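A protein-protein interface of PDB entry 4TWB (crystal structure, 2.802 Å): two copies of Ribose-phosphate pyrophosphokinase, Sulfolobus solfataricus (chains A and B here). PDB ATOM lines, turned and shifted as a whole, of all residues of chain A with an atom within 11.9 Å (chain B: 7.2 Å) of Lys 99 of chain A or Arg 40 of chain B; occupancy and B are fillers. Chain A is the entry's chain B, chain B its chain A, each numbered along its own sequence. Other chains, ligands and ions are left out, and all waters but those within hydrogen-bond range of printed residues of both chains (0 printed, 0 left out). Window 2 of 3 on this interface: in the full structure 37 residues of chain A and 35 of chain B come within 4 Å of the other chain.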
ATOM      1  N   TYR A  91     -20.765 -18.736 -15.033  1.00  0.00           N
ATOM      2  CA  TYR A  91     -19.604 -17.904 -15.347  1.00  0.00           C
ATOM      3  C   TYR A  91     -20.000 -16.633 -16.105  1.00  0.00           C
ATOM      4  O   TYR A  91     -19.207 -16.072 -16.856  1.00  0.00           O
ATOM      5  CB  TYR A  91     -18.509 -18.722 -16.060  1.00  0.00           C
ATOM      6  CG  TYR A  91     -17.882 -19.742 -15.122  1.00  0.00           C
ATOM      7  CD1 TYR A  91     -16.808 -19.401 -14.326  1.00  0.00           C
ATOM      8  CD2 TYR A  91     -18.411 -21.021 -14.990  1.00  0.00           C
ATOM      9  CE1 TYR A  91     -16.264 -20.298 -13.454  1.00  0.00           C
ATOM     10  CE2 TYR A  91     -17.874 -21.919 -14.117  1.00  0.00           C
ATOM     11  CZ  TYR A  91     -16.803 -21.553 -13.352  1.00  0.00           C
ATOM     12  OH  TYR A  91     -16.253 -22.443 -12.472  1.00  0.00           O
ATOM     13  N   ARG A  93     -21.113 -13.824 -14.477  1.00  0.00           N
ATOM     14  CA  ARG A  93     -20.668 -12.664 -13.720  1.00  0.00           C
ATOM     15  C   ARG A  93     -19.234 -12.266 -14.115  1.00  0.00           C
ATOM     16  O   ARG A  93     -18.810 -11.132 -13.879  1.00  0.00           O
ATOM     17  CB  ARG A  93     -20.792 -12.927 -12.218  1.00  0.00           C
ATOM     18  CG  ARG A  93     -22.236 -12.971 -11.697  1.00  0.00           C
ATOM     19  CD  ARG A  93     -22.461 -14.223 -10.815  1.00  0.00           C
ATOM     20  NE  ARG A  93     -23.049 -13.959  -9.496  1.00  0.00           N
ATOM     21  CZ  ARG A  93     -22.834 -12.867  -8.762  1.00  0.00           C
ATOM     22  NH1 ARG A  93     -22.031 -11.903  -9.194  1.00  0.00           N
ATOM     23  NH2 ARG A  93     -23.419 -12.740  -7.579  1.00  0.00           N
ATOM     24  N   GLN A  94     -18.504 -13.186 -14.746  1.00  0.00           N
ATOM     25  CA  GLN A  94     -17.126 -12.907 -15.167  1.00  0.00           C
ATOM     26  C   GLN A  94     -17.057 -12.373 -16.592  1.00  0.00           C
ATOM     27  O   GLN A  94     -16.734 -13.097 -17.536  1.00  0.00           O
ATOM     28  CB  GLN A  94     -16.239 -14.140 -15.031  1.00  0.00           C
ATOM     29  CG  GLN A  94     -14.767 -13.849 -15.286  1.00  0.00           C
ATOM     30  CD  GLN A  94     -14.124 -13.009 -14.191  1.00  0.00           C
ATOM     31  OE1 GLN A  94     -14.726 -12.746 -13.140  1.00  0.00           O
ATOM     32  NE2 GLN A  94     -12.883 -12.594 -14.429  1.00  0.00           N
ATOM     33  N   ASP A  95     -17.332 -11.080 -16.714  1.00  0.00           N
ATOM     34  CA  ASP A  95     -17.603 -10.407 -17.985  1.00  0.00           C
ATOM     35  C   ASP A  95     -16.329  -9.970 -18.729  1.00  0.00           C
ATOM     36  O   ASP A  95     -16.307  -9.901 -19.964  1.00  0.00           O
ATOM     37  CB  ASP A  95     -18.486  -9.184 -17.684  1.00  0.00           C
ATOM     38  CG  ASP A  95     -19.336  -8.766 -18.860  1.00  0.00           C
ATOM     39  OD1 ASP A  95     -19.072  -9.233 -19.993  1.00  0.00           O
ATOM     40  OD2 ASP A  95     -20.269  -7.964 -18.642  1.00  0.00           O
ATOM     41  N   ARG A  96     -15.275  -9.684 -17.963  1.00  0.00           N
ATOM     42  CA  ARG A  96     -14.074  -9.035 -18.475  1.00  0.00           C
ATOM     43  C   ARG A  96     -12.944  -9.230 -17.485  1.00  0.00           C
ATOM     44  O   ARG A  96     -13.123  -9.902 -16.474  1.00  0.00           O
ATOM     45  CB  ARG A  96     -14.333  -7.536 -18.638  1.00  0.00           C
ATOM     46  CG  ARG A  96     -14.979  -6.874 -17.402  1.00  0.00           C
ATOM     47  CD  ARG A  96     -15.476  -5.445 -17.690  1.00  0.00           C
ATOM     48  NE  ARG A  96     -16.521  -5.029 -16.752  1.00  0.00           N
ATOM     49  CZ  ARG A  96     -17.814  -4.938 -17.058  1.00  0.00           C
ATOM     50  NH1 ARG A  96     -18.233  -5.217 -18.286  1.00  0.00           N
ATOM     51  NH2 ARG A  96     -18.690  -4.560 -16.137  1.00  0.00           N
ATOM     52  N   ARG A  97     -11.790  -8.630 -17.763  1.00  0.00           N
ATOM     53  CA  ARG A  97     -10.665  -8.680 -16.830  1.00  0.00           C
ATOM     54  C   ARG A  97     -10.705  -7.519 -15.835  1.00  0.00           C
ATOM     55  O   ARG A  97     -10.226  -6.422 -16.122  1.00  0.00           O
ATOM     56  CB  ARG A  97      -9.318  -8.693 -17.570  1.00  0.00           C
ATOM     57  CG  ARG A  97      -9.179  -9.802 -18.609  1.00  0.00           C
ATOM     58  CD  ARG A  97      -7.720 -10.127 -18.962  1.00  0.00           C
ATOM     59  NE  ARG A  97      -7.636 -10.715 -20.299  1.00  0.00           N
ATOM     60  CZ  ARG A  97      -7.851 -12.001 -20.584  1.00  0.00           C
ATOM     61  NH1 ARG A  97      -8.162 -12.856 -19.615  1.00  0.00           N
ATOM     62  NH2 ARG A  97      -7.753 -12.436 -21.837  1.00  0.00           N
ATOM     63  N   PHE A  98     -11.269  -7.770 -14.659  1.00  0.00           N
ATOM     64  CA  PHE A  98     -11.357  -6.752 -13.614  1.00  0.00           C
ATOM     65  C   PHE A  98      -9.979  -6.400 -13.031  1.00  0.00           C
ATOM     66  O   PHE A  98      -9.773  -5.296 -12.518  1.00  0.00           O
ATOM     67  CB  PHE A  98     -12.340  -7.187 -12.518  1.00  0.00           C
ATOM     68  CG  PHE A  98     -13.711  -7.531 -13.042  1.00  0.00           C
ATOM     69  CD1 PHE A  98     -14.663  -6.541 -13.226  1.00  0.00           C
ATOM     70  CD2 PHE A  98     -14.043  -8.844 -13.366  1.00  0.00           C
ATOM     71  CE1 PHE A  98     -15.923  -6.848 -13.714  1.00  0.00           C
ATOM     72  CE2 PHE A  98     -15.302  -9.162 -13.856  1.00  0.00           C
ATOM     73  CZ  PHE A  98     -16.245  -8.159 -14.030  1.00  0.00           C
ATOM     74  N   LYS A  99      -9.046  -7.345 -13.110  1.00  0.00           N
ATOM     75  CA  LYS A  99      -7.637  -7.085 -12.821  1.00  0.00           C
ATOM     76  C   LYS A  99      -6.843  -7.716 -13.952  1.00  0.00           C
ATOM     77  O   LYS A  99      -7.375  -8.547 -14.678  1.00  0.00           O
ATOM     78  CB  LYS A  99      -7.231  -7.689 -11.474  1.00  0.00           C
ATOM     79  CG  LYS A  99      -8.131  -7.289 -10.300  1.00  0.00           C
ATOM     80  CD  LYS A  99      -7.572  -7.794  -8.975  1.00  0.00           C
ATOM     81  CE  LYS A  99      -8.467  -7.413  -7.801  1.00  0.00           C
ATOM     82  NZ  LYS A  99      -7.938  -7.922  -6.497  1.00  0.00           N
ATOM     83  N   ASP A 100      -5.588  -7.326 -14.132  1.00  0.00           N
ATOM     84  CA  ASP A 100      -4.810  -7.894 -15.230  1.00  0.00           C
ATOM     85  C   ASP A 100      -4.484  -9.363 -14.971  1.00  0.00           C
ATOM     86  O   ASP A 100      -4.103  -9.730 -13.854  1.00  0.00           O
ATOM     87  CB  ASP A 100      -3.545  -7.075 -15.517  1.00  0.00           C
ATOM     88  CG  ASP A 100      -3.212  -6.101 -14.400  1.00  0.00           C
ATOM     89  OD1 ASP A 100      -3.295  -6.491 -13.213  1.00  0.00           O
ATOM     90  OD2 ASP A 100      -2.865  -4.939 -14.716  1.00  0.00           O
ATOM     91  N   GLY A 101      -4.668 -10.191 -16.001  1.00  0.00           N
ATOM     92  CA  GLY A 101      -4.424 -11.615 -15.899  1.00  0.00           C
ATOM     93  C   GLY A 101      -5.571 -12.440 -15.335  1.00  0.00           C
ATOM     94  O   GLY A 101      -5.452 -13.659 -15.162  1.00  0.00           O
ATOM     95  N   GLU A 102      -6.684 -11.789 -15.024  1.00  0.00           N
ATOM     96  CA  GLU A 102      -7.894 -12.534 -14.686  1.00  0.00           C
ATOM     97  C   GLU A 102      -8.410 -13.203 -15.954  1.00  0.00           C
ATOM     98  O   GLU A 102      -8.207 -12.698 -17.060  1.00  0.00           O
ATOM     99  CB  GLU A 102      -8.981 -11.625 -14.106  1.00  0.00           C
ATOM    100  CG  GLU A 102      -8.884 -11.354 -12.604  1.00  0.00           C
ATOM    101  CD  GLU A 102     -10.058 -10.520 -12.115  1.00  0.00           C
ATOM    102  OE1 GLU A 102     -10.954 -10.245 -12.941  1.00  0.00           O
ATOM    103  OE2 GLU A 102     -10.086 -10.136 -10.922  1.00  0.00           O
ATOM    104  N   ALA A 103      -9.068 -14.345 -15.784  1.00  0.00           N
ATOM    105  CA  ALA A 103      -9.674 -15.051 -16.900  1.00  0.00           C
ATOM    106  C   ALA A 103     -11.001 -14.420 -17.267  1.00  0.00           C
ATOM    107  O   ALA A 103     -11.789 -14.022 -16.411  1.00  0.00           O
ATOM    108  CB  ALA A 103      -9.886 -16.502 -16.548  1.00  0.00           C
ATOM    109  N   ILE A 104     -11.259 -14.323 -18.555  1.00  0.00           N
ATOM    110  CA  ILE A 104     -12.594 -13.971 -18.985  1.00  0.00           C
ATOM    111  C   ILE A 104     -13.366 -15.275 -19.158  1.00  0.00           C
ATOM    112  O   ILE A 104     -13.498 -15.794 -20.279  1.00  0.00           O
ATOM    113  CB  ILE A 104     -12.558 -13.175 -20.292  1.00  0.00           C
ATOM    114  CG1 ILE A 104     -11.611 -11.989 -20.131  1.00  0.00           C
ATOM    115  CG2 ILE A 104     -13.947 -12.690 -20.653  1.00  0.00           C
ATOM    116  CD1 ILE A 104     -11.282 -11.277 -21.412  1.00  0.00           C
ATOM    117  N   SER A 105     -13.857 -15.807 -18.039  1.00  0.00           N
ATOM    118  CA  SER A 105     -14.478 -17.135 -18.001  1.00  0.00           C
ATOM    119  C   SER A 105     -15.557 -17.318 -19.068  1.00  0.00           C
ATOM    120  O   SER A 105     -15.620 -18.348 -19.749  1.00  0.00           O
ATOM    121  CB  SER A 105     -15.065 -17.421 -16.619  1.00  0.00           C
ATOM    122  OG  SER A 105     -14.143 -17.117 -15.576  1.00  0.00           O
ATOM    123  N   THR A 108     -14.291 -18.213 -22.614  1.00  0.00           N
ATOM    124  CA  THR A 108     -13.871 -19.598 -22.746  1.00  0.00           C
ATOM    125  C   THR A 108     -15.070 -20.523 -22.874  1.00  0.00           C
ATOM    126  O   THR A 108     -15.129 -21.376 -23.756  1.00  0.00           O
ATOM    127  CB  THR A 108     -13.056 -20.039 -21.518  1.00  0.00           C
ATOM    128  OG1 THR A 108     -11.913 -19.181 -21.343  1.00  0.00           O
ATOM    129  CG2 THR A 108     -12.604 -21.451 -21.700  1.00  0.00           C
ATOM    130  N   ILE B   4       3.929 -22.486 -14.919  1.00  0.00           N
ATOM    131  CA  ILE B   4       2.769 -21.960 -14.225  1.00  0.00           C
ATOM    132  C   ILE B   4       2.063 -23.090 -13.532  1.00  0.00           C
ATOM    133  O   ILE B   4       1.631 -24.031 -14.180  1.00  0.00           O
ATOM    134  CB  ILE B   4       1.777 -21.260 -15.174  1.00  0.00           C
ATOM    135  CG1 ILE B   4       2.444 -20.060 -15.852  1.00  0.00           C
ATOM    136  CG2 ILE B   4       0.563 -20.798 -14.393  1.00  0.00           C
ATOM    137  CD1 ILE B   4       1.625 -19.453 -16.947  1.00  0.00           C
ATOM    138  N   VAL B  25       5.717 -19.633 -11.465  1.00  0.00           N
ATOM    139  CA  VAL B  25       4.640 -18.669 -11.258  1.00  0.00           C
ATOM    140  C   VAL B  25       3.345 -19.392 -10.894  1.00  0.00           C
ATOM    141  O   VAL B  25       2.834 -20.193 -11.678  1.00  0.00           O
ATOM    142  CB  VAL B  25       4.412 -17.851 -12.529  1.00  0.00           C
ATOM    143  CG1 VAL B  25       3.092 -17.115 -12.458  1.00  0.00           C
ATOM    144  CG2 VAL B  25       5.571 -16.893 -12.746  1.00  0.00           C
ATOM    145  N   LYS B  26       2.814 -19.113  -9.707  1.00  0.00           N
ATOM    146  CA  LYS B  26       1.577 -19.762  -9.255  1.00  0.00           C
ATOM    147  C   LYS B  26       0.296 -18.997  -9.622  1.00  0.00           C
ATOM    148  O   LYS B  26       0.179 -17.792  -9.369  1.00  0.00           O
ATOM    149  CB  LYS B  26       1.615 -20.031  -7.743  1.00  0.00           C
ATOM    150  CG  LYS B  26       2.549 -21.168  -7.345  1.00  0.00           C
ATOM    151  CD  LYS B  26       1.895 -22.065  -6.309  1.00  0.00           C
ATOM    152  CE  LYS B  26       2.657 -23.381  -6.151  1.00  0.00           C
ATOM    153  NZ  LYS B  26       1.821 -24.488  -5.577  1.00  0.00           N
ATOM    154  N   VAL B  27      -0.662 -19.712 -10.214  1.00  0.00           N
ATOM    155  CA  VAL B  27      -1.978 -19.151 -10.539  1.00  0.00           C
ATOM    156  C   VAL B  27      -2.794 -18.828  -9.279  1.00  0.00           C
ATOM    157  O   VAL B  27      -2.930 -19.651  -8.373  1.00  0.00           O
ATOM    158  CB  VAL B  27      -2.797 -20.109 -11.433  1.00  0.00           C
ATOM    159  CG1 VAL B  27      -4.280 -19.854 -11.278  1.00  0.00           C
ATOM    160  CG2 VAL B  27      -2.390 -19.965 -12.875  1.00  0.00           C
ATOM    161  N   GLU B  28      -3.325 -17.616  -9.223  1.00  0.00           N
ATOM    162  CA  GLU B  28      -4.210 -17.230  -8.131  1.00  0.00           C
ATOM    163  C   GLU B  28      -5.579 -17.852  -8.394  1.00  0.00           C
ATOM    164  O   GLU B  28      -6.140 -17.728  -9.493  1.00  0.00           O
ATOM    165  CB  GLU B  28      -4.313 -15.704  -8.037  1.00  0.00           C
ATOM    166  CG  GLU B  28      -5.076 -15.187  -6.825  1.00  0.00           C
ATOM    167  CD  GLU B  28      -5.246 -13.661  -6.835  1.00  0.00           C
ATOM    168  OE1 GLU B  28      -4.590 -12.972  -7.659  1.00  0.00           O
ATOM    169  OE2 GLU B  28      -6.041 -13.155  -6.009  1.00  0.00           O
ATOM    170  N   ASN B  29      -6.117 -18.545  -7.401  1.00  0.00           N
ATOM    171  CA  ASN B  29      -7.385 -19.215  -7.616  1.00  0.00           C
ATOM    172  C   ASN B  29      -8.203 -19.345  -6.337  1.00  0.00           C
ATOM    173  O   ASN B  29      -7.680 -19.740  -5.294  1.00  0.00           O
ATOM    174  CB  ASN B  29      -7.157 -20.579  -8.272  1.00  0.00           C
ATOM    175  CG  ASN B  29      -7.164 -21.718  -7.277  1.00  0.00           C
ATOM    176  OD1 ASN B  29      -6.113 -22.101  -6.739  1.00  0.00           O
ATOM    177  ND2 ASN B  29      -8.355 -22.275  -7.026  1.00  0.00           N
ATOM    178  N   LYS B  30      -9.482 -18.979  -6.418  1.00  0.00           N
ATOM    179  CA  LYS B  30     -10.398 -19.111  -5.285  1.00  0.00           C
ATOM    180  C   LYS B  30     -11.770 -19.556  -5.766  1.00  0.00           C
ATOM    181  O   LYS B  30     -12.036 -19.587  -6.967  1.00  0.00           O
ATOM    182  CB  LYS B  30     -10.517 -17.797  -4.493  1.00  0.00           C
ATOM    183  CG  LYS B  30     -10.671 -16.541  -5.350  1.00  0.00           C
ATOM    184  CD  LYS B  30     -11.249 -15.360  -4.544  1.00  0.00           C
ATOM    185  CE  LYS B  30     -11.515 -14.140  -5.440  1.00  0.00           C
ATOM    186  NZ  LYS B  30     -12.518 -13.196  -4.883  1.00  0.00           N
ATOM    187  N   TYR B  38     -12.595 -18.787  -9.575  1.00  0.00           N
ATOM    188  CA  TYR B  38     -11.879 -17.562  -9.907  1.00  0.00           C
ATOM    189  C   TYR B  38     -10.456 -17.907 -10.329  1.00  0.00           C
ATOM    190  O   TYR B  38      -9.777 -18.688  -9.672  1.00  0.00           O
ATOM    191  CB  TYR B  38     -11.846 -16.607  -8.712  1.00  0.00           C
ATOM    192  CG  TYR B  38     -11.032 -15.363  -8.964  1.00  0.00           C
ATOM    193  CD1 TYR B  38     -11.533 -14.331  -9.746  1.00  0.00           C
ATOM    194  CD2 TYR B  38      -9.763 -15.218  -8.418  1.00  0.00           C
ATOM    195  CE1 TYR B  38     -10.789 -13.183  -9.982  1.00  0.00           C
ATOM    196  CE2 TYR B  38      -9.007 -14.079  -8.647  1.00  0.00           C
ATOM    197  CZ  TYR B  38      -9.526 -13.062  -9.429  1.00  0.00           C
ATOM    198  OH  TYR B  38      -8.779 -11.926  -9.659  1.00  0.00           O
ATOM    199  N   ILE B  39     -10.004 -17.300 -11.420  1.00  0.00           N
ATOM    200  CA  ILE B  39      -8.718 -17.636 -12.014  1.00  0.00           C
ATOM    201  C   ILE B  39      -7.960 -16.386 -12.455  1.00  0.00           C
ATOM    202  O   ILE B  39      -8.455 -15.613 -13.270  1.00  0.00           O
ATOM    203  CB  ILE B  39      -8.916 -18.552 -13.250  1.00  0.00           C
ATOM    204  CG1 ILE B  39      -9.435 -19.928 -12.816  1.00  0.00           C
ATOM    205  CG2 ILE B  39      -7.626 -18.673 -14.053  1.00  0.00           C
ATOM    206  CD1 ILE B  39      -8.486 -20.690 -11.944  1.00  0.00           C
ATOM    207  N   ARG B  40      -6.754 -16.201 -11.924  1.00  0.00           N
ATOM    208  CA  ARG B  40      -5.893 -15.090 -12.331  1.00  0.00           C
ATOM    209  C   ARG B  40      -4.423 -15.508 -12.530  1.00  0.00           C
ATOM    210  O   ARG B  40      -3.824 -16.137 -11.660  1.00  0.00           O
ATOM    211  CB  ARG B  40      -5.960 -13.965 -11.304  1.00  0.00           C
ATOM    212  CG  ARG B  40      -5.392 -12.658 -11.820  1.00  0.00           C
ATOM    213  CD  ARG B  40      -5.029 -11.728 -10.681  1.00  0.00           C
ATOM    214  NE  ARG B  40      -4.351 -10.534 -11.176  1.00  0.00           N
ATOM    215  CZ  ARG B  40      -4.035  -9.484 -10.425  1.00  0.00           C
ATOM    216  NH1 ARG B  40      -4.336  -9.474  -9.131  1.00  0.00           N
ATOM    217  NH2 ARG B  40      -3.422  -8.439 -10.969  1.00  0.00           N
ATOM    218  N   VAL B  41      -3.842 -15.135 -13.668  1.00  0.00           N
ATOM    219  CA  VAL B  41      -2.449 -15.459 -13.979  1.00  0.00           C
ATOM    220  C   VAL B  41      -1.531 -14.269 -13.701  1.00  0.00           C
ATOM    221  O   VAL B  41      -1.425 -13.357 -14.527  1.00  0.00           O
ATOM    222  CB  VAL B  41      -2.298 -15.853 -15.449  1.00  0.00           C
ATOM    223  CG1 VAL B  41      -0.838 -16.144 -15.758  1.00  0.00           C
ATOM    224  CG2 VAL B  41      -3.174 -17.054 -15.775  1.00  0.00           C
ATOM    225  N   PRO B  42      -0.825 -14.304 -12.554  1.00  0.00           N
ATOM    226  CA  PRO B  42      -0.339 -13.116 -11.830  1.00  0.00           C
ATOM    227  C   PRO B  42       0.925 -12.445 -12.365  1.00  0.00           C
ATOM    228  O   PRO B  42       1.377 -11.472 -11.751  1.00  0.00           O
ATOM    229  CB  PRO B  42      -0.060 -13.651 -10.411  1.00  0.00           C
ATOM    230  CG  PRO B  42      -0.420 -15.135 -10.439  1.00  0.00           C
ATOM    231  CD  PRO B  42      -0.402 -15.541 -11.887  1.00  0.00           C
ATOM    232  N   SER B  43       1.486 -12.934 -13.466  1.00  0.00           N
ATOM    233  CA  SER B  43       2.707 -12.319 -13.988  1.00  0.00           C
ATOM    234  C   SER B  43       2.547 -11.788 -15.399  1.00  0.00           C
ATOM    235  O   SER B  43       1.455 -11.818 -15.979  1.00  0.00           O
ATOM    236  CB  SER B  43       3.894 -13.300 -13.949  1.00  0.00           C
ATOM    237  OG  SER B  43       4.751 -13.072 -12.833  1.00  0.00           O
ATOM    238  N   ILE B  70      -7.630 -21.315 -17.370  1.00  0.00           N
ATOM    239  CA  ILE B  70      -6.228 -20.958 -17.243  1.00  0.00           C
ATOM    240  C   ILE B  70      -5.540 -21.002 -18.612  1.00  0.00           C
ATOM    241  O   ILE B  70      -4.759 -20.116 -18.962  1.00  0.00           O
ATOM    242  CB  ILE B  70      -5.499 -21.905 -16.287  1.00  0.00           C
ATOM    243  CG1 ILE B  70      -6.053 -21.753 -14.871  1.00  0.00           C
ATOM    244  CG2 ILE B  70      -3.988 -21.647 -16.317  1.00  0.00           C
ATOM    245  CD1 ILE B  70      -5.622 -22.840 -13.918  1.00  0.00           C
ATOM    246  N   THR B  73      -6.586 -17.965 -20.824  1.00  0.00           N
ATOM    247  CA  THR B  73      -5.944 -16.804 -20.221  1.00  0.00           C
ATOM    248  C   THR B  73      -4.465 -16.696 -20.606  1.00  0.00           C
ATOM    249  O   THR B  73      -3.987 -15.622 -20.977  1.00  0.00           O
ATOM    250  CB  THR B  73      -6.046 -16.851 -18.686  1.00  0.00           C
ATOM    251  OG1 THR B  73      -7.419 -17.005 -18.292  1.00  0.00           O
ATOM    252  CG2 THR B  73      -5.473 -15.582 -18.071  1.00  0.00           C
ATOM    253  N   LEU B  77      -2.704 -13.892 -22.815  1.00  0.00           N
ATOM    254  CA  LEU B  77      -1.701 -13.017 -22.226  1.00  0.00           C
ATOM    255  C   LEU B  77      -0.405 -12.949 -23.039  1.00  0.00           C
ATOM    256  O   LEU B  77       0.587 -12.374 -22.583  1.00  0.00           O
ATOM    257  CB  LEU B  77      -1.398 -13.451 -20.797  1.00  0.00           C
ATOM    258  CG  LEU B  77      -2.435 -13.054 -19.744  1.00  0.00           C
ATOM    259  CD1 LEU B  77      -2.276 -13.911 -18.494  1.00  0.00           C
ATOM    260  CD2 LEU B  77      -2.285 -11.588 -19.405  1.00  0.00           C
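Among the printed residues, merely in contact across the chains: Ala 103 of chain A with Thr 73 of chain B, Gly 101 of chain A with Arg 40 of chain B, Glu 102 of chain A with Ile 39 of chain B, Gly 101 of chain A with Thr 73 of chain B, Glu 102 of chain A with Arg 40 of chain B and Lys 99 of chain A with Arg 40 of chain B.
N of Tyr 38 of chain B is in hydrogen-bond range of O of Lys 30 of chain B. The backbone carbonyl oxygen (O) of Ala 103 of chain A sits at hydrogen-bond distance from the side-chain amide nitrogen (NE2) of Gln 94 of chain A, at 2.7 Å. The backbone NH (N) of Lys 99 of chain A is in hydrogen-bond range of the side-chain carboxylate (OE1) of Glu 102 of chain A (3.5 Å). The side-chain amide nitrogen (NE2) of Gln 94 of chain A is in hydrogen-bond range of the side-chain carboxylate (OE1) of Glu 102 of chain A, at 3.4 Å. The side-chain carboxylate of Glu 102 of chain A is in hydrogen-bond range of the backbone NH of Phe 98 of chain A, 3.0 Å away. OE1 of Glu 28 of chain B lies within salt-bridge range of NH1 of Arg 40 of chain B, 3.8 Å away.
Hydrophobic or aromatic side chains of chain A that line the printed part of chain B: Ala 103. Along chain A the printed residues that touch a printed residue of chain B span positions 99 to 103. Of the 16 printed residues of chain B, 5 touch a printed residue of chain A. Along chain B the printed residues that touch a printed residue of chain A span positions 38 to 73. Among the printed residues, Asp or Glu carboxylates within 4 Å of a Lys or Arg side-chain nitrogen of the other chain: Asp 100 of chain A with Arg 40 of chain B.
No position is printed for both chains. Of the 10 pairs that touch across the chains among the printed residues, none has its exchanged pair printed and touching as well.
OD1 of Asp 100 of chain A lies within salt-bridge range of NH2 of Arg 40 of chain B (3.0 Å). OH of Tyr 38 of chain B lies within hydrogen-bond range of OE2 of Glu 102 of chain A (2.6 Å). The backbone NH of Ala 103 of chain A is in hydrogen-bond range of the backbone carbonyl oxygen of Ile 39 of chain B, 2.9 Å away. The backbone NH of Val 41 of chain B sits at hydrogen-bond distance from the backbone carbonyl oxygen of Gly 101 of chain A.
Lys 99 of chain A touches just one residue of chain B: Arg 40. No residue of chain A comes within 4 Å of Val 27 of chain B. Of chain A, only Glu 102 comes within 4 Å of Tyr 38 of chain B. Printed residues of chain A within 4 Å of Val 41 of chain B: Gly 101. Pro 42 of chain B touches none of the printed residues of chain A. Of the printed residues of chain B, Gly 101 of chain A touches Arg 40, Val 41 and Thr 73. Printed residues of chain A within 4 Å of Thr 73 of chain B: Gly 101 (3.5 Å) and Ala 103 (3.1 Å). Of the printed residues of chain B, Ala 103 of chain A touches Ile 39 (2.9 Å) and Thr 73 (3.1 Å). Of the printed residues of chain B, Asp 100 of chain A touches Arg 40. Of the printed residues of chain B, Glu 102 of chain A touches Tyr 38, Ile 39 and Arg 40. The nearest residue of chain B that does not touch Lys 99 of chain A is Tyr 38 of chain B (4.4 Å).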
